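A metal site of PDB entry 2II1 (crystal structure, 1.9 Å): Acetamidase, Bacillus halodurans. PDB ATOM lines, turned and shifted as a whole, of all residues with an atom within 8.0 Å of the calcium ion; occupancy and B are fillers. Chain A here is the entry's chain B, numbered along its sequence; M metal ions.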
ATOM      1  N   ALA A 247      -2.740 -13.184  18.298  1.00  0.00           N
ATOM      2  CA  ALA A 247      -3.170 -12.995  19.709  1.00  0.00           C
ATOM      3  C   ALA A 247      -3.621 -14.309  20.351  1.00  0.00           C
ATOM      4  O   ALA A 247      -3.221 -14.672  21.450  1.00  0.00           O
ATOM      5  CB  ALA A 247      -4.335 -11.971  19.788  1.00  0.00           C
ATOM      6  N   THR A 248      -4.484 -15.029  19.667  1.00  0.00           N
ATOM      7  CA  THR A 248      -5.017 -16.241  20.213  1.00  0.00           C
ATOM      8  C   THR A 248      -3.929 -17.323  20.329  1.00  0.00           C
ATOM      9  O   THR A 248      -3.915 -18.031  21.324  1.00  0.00           O
ATOM     10  CB  THR A 248      -6.201 -16.752  19.384  1.00  0.00           C
ATOM     11  OG1 THR A 248      -5.791 -16.903  18.021  1.00  0.00           O
ATOM     12  CG2 THR A 248      -7.357 -15.796  19.466  1.00  0.00           C
ATOM     13  N   PHE A 249      -3.045 -17.427  19.333  1.00  0.00           N
ATOM     14  CA  PHE A 249      -1.839 -18.278  19.405  1.00  0.00           C
ATOM     15  C   PHE A 249      -0.898 -17.944  20.603  1.00  0.00           C
ATOM     16  O   PHE A 249      -0.482 -18.828  21.361  1.00  0.00           O
ATOM     17  CB  PHE A 249      -1.060 -18.197  18.077  1.00  0.00           C
ATOM     18  CG  PHE A 249       0.316 -18.818  18.121  1.00  0.00           C
ATOM     19  CD1 PHE A 249       0.491 -20.123  18.579  1.00  0.00           C
ATOM     20  CD2 PHE A 249       1.429 -18.114  17.697  1.00  0.00           C
ATOM     21  CE1 PHE A 249       1.765 -20.710  18.635  1.00  0.00           C
ATOM     22  CE2 PHE A 249       2.705 -18.697  17.740  1.00  0.00           C
ATOM     23  CZ  PHE A 249       2.874 -19.995  18.220  1.00  0.00           C
ATOM     24  N   LEU A 250      -0.572 -16.667  20.744  1.00  0.00           N
ATOM     25  CA  LEU A 250       0.295 -16.188  21.812  1.00  0.00           C
ATOM     26  C   LEU A 250      -0.390 -16.313  23.205  1.00  0.00           C
ATOM     27  O   LEU A 250       0.261 -16.629  24.189  1.00  0.00           O
ATOM     28  CB  LEU A 250       0.736 -14.747  21.442  1.00  0.00           C
ATOM     29  CG  LEU A 250       1.766 -13.877  22.169  1.00  0.00           C
ATOM     30  CD1 LEU A 250       3.173 -14.491  22.199  1.00  0.00           C
ATOM     31  CD2 LEU A 250       1.786 -12.512  21.472  1.00  0.00           C
ATOM     32  N   ALA A 251      -1.707 -16.132  23.288  1.00  0.00           N
ATOM     33  CA  ALA A 251      -2.418 -16.395  24.533  1.00  0.00           C
ATOM     34  C   ALA A 251      -2.412 -17.884  24.802  1.00  0.00           C
ATOM     35  O   ALA A 251      -2.028 -18.341  25.879  1.00  0.00           O
ATOM     36  CB  ALA A 251      -3.843 -15.862  24.478  1.00  0.00           C
ATOM     37  N   ASN A 252      -2.862 -18.659  23.811  1.00  0.00           N
ATOM     38  CA  ASN A 252      -2.979 -20.106  23.957  1.00  0.00           C
ATOM     39  C   ASN A 252      -1.681 -20.819  24.350  1.00  0.00           C
ATOM     40  O   ASN A 252      -1.711 -21.717  25.168  1.00  0.00           O
ATOM     41  CB  ASN A 252      -3.547 -20.758  22.679  1.00  0.00           C
ATOM     42  CG  ASN A 252      -5.034 -20.453  22.458  1.00  0.00           C
ATOM     43  OD1 ASN A 252      -5.785 -20.208  23.388  1.00  0.00           O
ATOM     44  ND2 ASN A 252      -5.463 -20.480  21.196  1.00  0.00           N
ATOM     45  N   ARG A 253      -0.556 -20.409  23.775  1.00  0.00           N
ATOM     46  CA  ARG A 253       0.721 -21.130  23.936  1.00  0.00           C
ATOM     47  C   ARG A 253       1.672 -20.553  24.987  1.00  0.00           C
ATOM     48  O   ARG A 253       2.731 -21.144  25.254  1.00  0.00           O
ATOM     49  CB  ARG A 253       1.441 -21.242  22.589  1.00  0.00           C
ATOM     50  CG  ARG A 253       0.827 -22.286  21.642  1.00  0.00           C
ATOM     51  N   THR A 254       1.288 -19.446  25.623  1.00  0.00           N
ATOM     52  CA  THR A 254       2.122 -18.714  26.568  1.00  0.00           C
ATOM     53  C   THR A 254       1.390 -18.446  27.886  1.00  0.00           C
ATOM     54  O   THR A 254       0.141 -18.524  27.965  1.00  0.00           O
ATOM     55  CB  THR A 254       2.537 -17.317  25.973  1.00  0.00           C
ATOM     56  OG1 THR A 254       2.966 -17.462  24.599  1.00  0.00           O
ATOM     57  CG2 THR A 254       3.647 -16.693  26.768  1.00  0.00           C
ATOM     58  N   ALA A 255       2.166 -18.060  28.890  1.00  0.00           N
ATOM     59  CA  ALA A 255       1.661 -17.618  30.171  1.00  0.00           C
ATOM     60  C   ALA A 255       0.864 -16.318  30.068  1.00  0.00           C
ATOM     61  O   ALA A 255       0.226 -15.909  31.020  1.00  0.00           O
ATOM     62  CB  ALA A 255       2.808 -17.428  31.135  1.00  0.00           C
ATOM     63  N   LEU A 256       0.901 -15.673  28.908  1.00  0.00           N
ATOM     64  CA  LEU A 256       0.161 -14.445  28.734  1.00  0.00           C
ATOM     65  C   LEU A 256      -1.325 -14.740  28.665  1.00  0.00           C
ATOM     66  O   LEU A 256      -1.726 -15.735  28.056  1.00  0.00           O
ATOM     67  CB  LEU A 256       0.567 -13.770  27.410  1.00  0.00           C
ATOM     68  CG  LEU A 256       2.000 -13.337  27.205  1.00  0.00           C
ATOM     69  CD1 LEU A 256       2.052 -12.536  25.890  1.00  0.00           C
ATOM     70  CD2 LEU A 256       2.560 -12.494  28.367  1.00  0.00           C
ATOM     71  N   SER A 257      -2.128 -13.847  29.232  1.00  0.00           N
ATOM     72  CA  SER A 257      -3.566 -13.792  28.977  1.00  0.00           C
ATOM     73  C   SER A 257      -3.826 -13.189  27.613  1.00  0.00           C
ATOM     74  O   SER A 257      -2.914 -12.643  26.977  1.00  0.00           O
ATOM     75  CB  SER A 257      -4.231 -12.922  30.024  1.00  0.00           C
ATOM     76  OG  SER A 257      -3.724 -11.603  29.904  1.00  0.00           O
ATOM     77  N   ILE A 258      -5.071 -13.262  27.168  1.00  0.00           N
ATOM     78  CA  ILE A 258      -5.473 -12.672  25.887  1.00  0.00           C
ATOM     79  C   ILE A 258      -5.323 -11.169  25.947  1.00  0.00           C
ATOM     80  O   ILE A 258      -5.000 -10.529  24.960  1.00  0.00           O
ATOM     81  CB  ILE A 258      -6.926 -13.082  25.486  1.00  0.00           C
ATOM     82  CG1 ILE A 258      -7.217 -12.715  24.018  1.00  0.00           C
ATOM     83  CG2 ILE A 258      -7.949 -12.508  26.464  1.00  0.00           C
ATOM     84  CD1 ILE A 258      -6.273 -13.396  22.991  1.00  0.00           C
ATOM     85  N   GLU A 260      -2.935  -9.630  27.901  1.00  0.00           N
ATOM     86  CA  GLU A 260      -1.492  -9.386  27.858  1.00  0.00           C
ATOM     87  C   GLU A 260      -0.921  -9.611  26.455  1.00  0.00           C
ATOM     88  O   GLU A 260      -0.046  -8.877  26.004  1.00  0.00           O
ATOM     89  CB  GLU A 260      -0.785 -10.283  28.859  1.00  0.00           C
ATOM     90  CG  GLU A 260      -1.062  -9.898  30.299  1.00  0.00           C
ATOM     91  CD  GLU A 260      -0.454 -10.849  31.281  1.00  0.00           C
ATOM     92  OE1 GLU A 260      -0.522 -12.054  31.044  1.00  0.00           O
ATOM     93  OE2 GLU A 260       0.081 -10.374  32.291  1.00  0.00           O
ATOM     94  N   ALA A 261      -1.447 -10.614  25.758  1.00  0.00           N
ATOM     95  CA  ALA A 261      -1.118 -10.830  24.338  1.00  0.00           C
ATOM     96  C   ALA A 261      -1.475  -9.601  23.462  1.00  0.00           C
ATOM     97  O   ALA A 261      -0.664  -9.143  22.660  1.00  0.00           O
ATOM     98  CB  ALA A 261      -1.805 -12.114  23.828  1.00  0.00           C
HETATM   99 CA    CA M   1      -2.238 -18.017  28.283  1.00  0.00          CA
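Merely in contact with the calcium ion: Ala 255 (3.96 Å).
Within 4 Å of the calcium ion: Ala 251, Thr 254, Ala 255 and Leu 256.
Along chain A the residues within 4 Å of the calcium ion span positions 251 to 256.
The nearest printed residue that does not touch the calcium ion is Ser 257 (4.3 Å).
The calcium ion is bound by the backbone carbonyl oxygen (O) of Leu 256, at 2.3 Å.
The backbone carbonyl oxygen (O) of Ala 251 binds the calcium ion (2.4 Å).
The calcium ion is bound by O of Thr 254, at 2.5 Å.
OG1 of Thr 254 lies within hydrogen-bond range of O of Leu 250 (2.9 Å).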
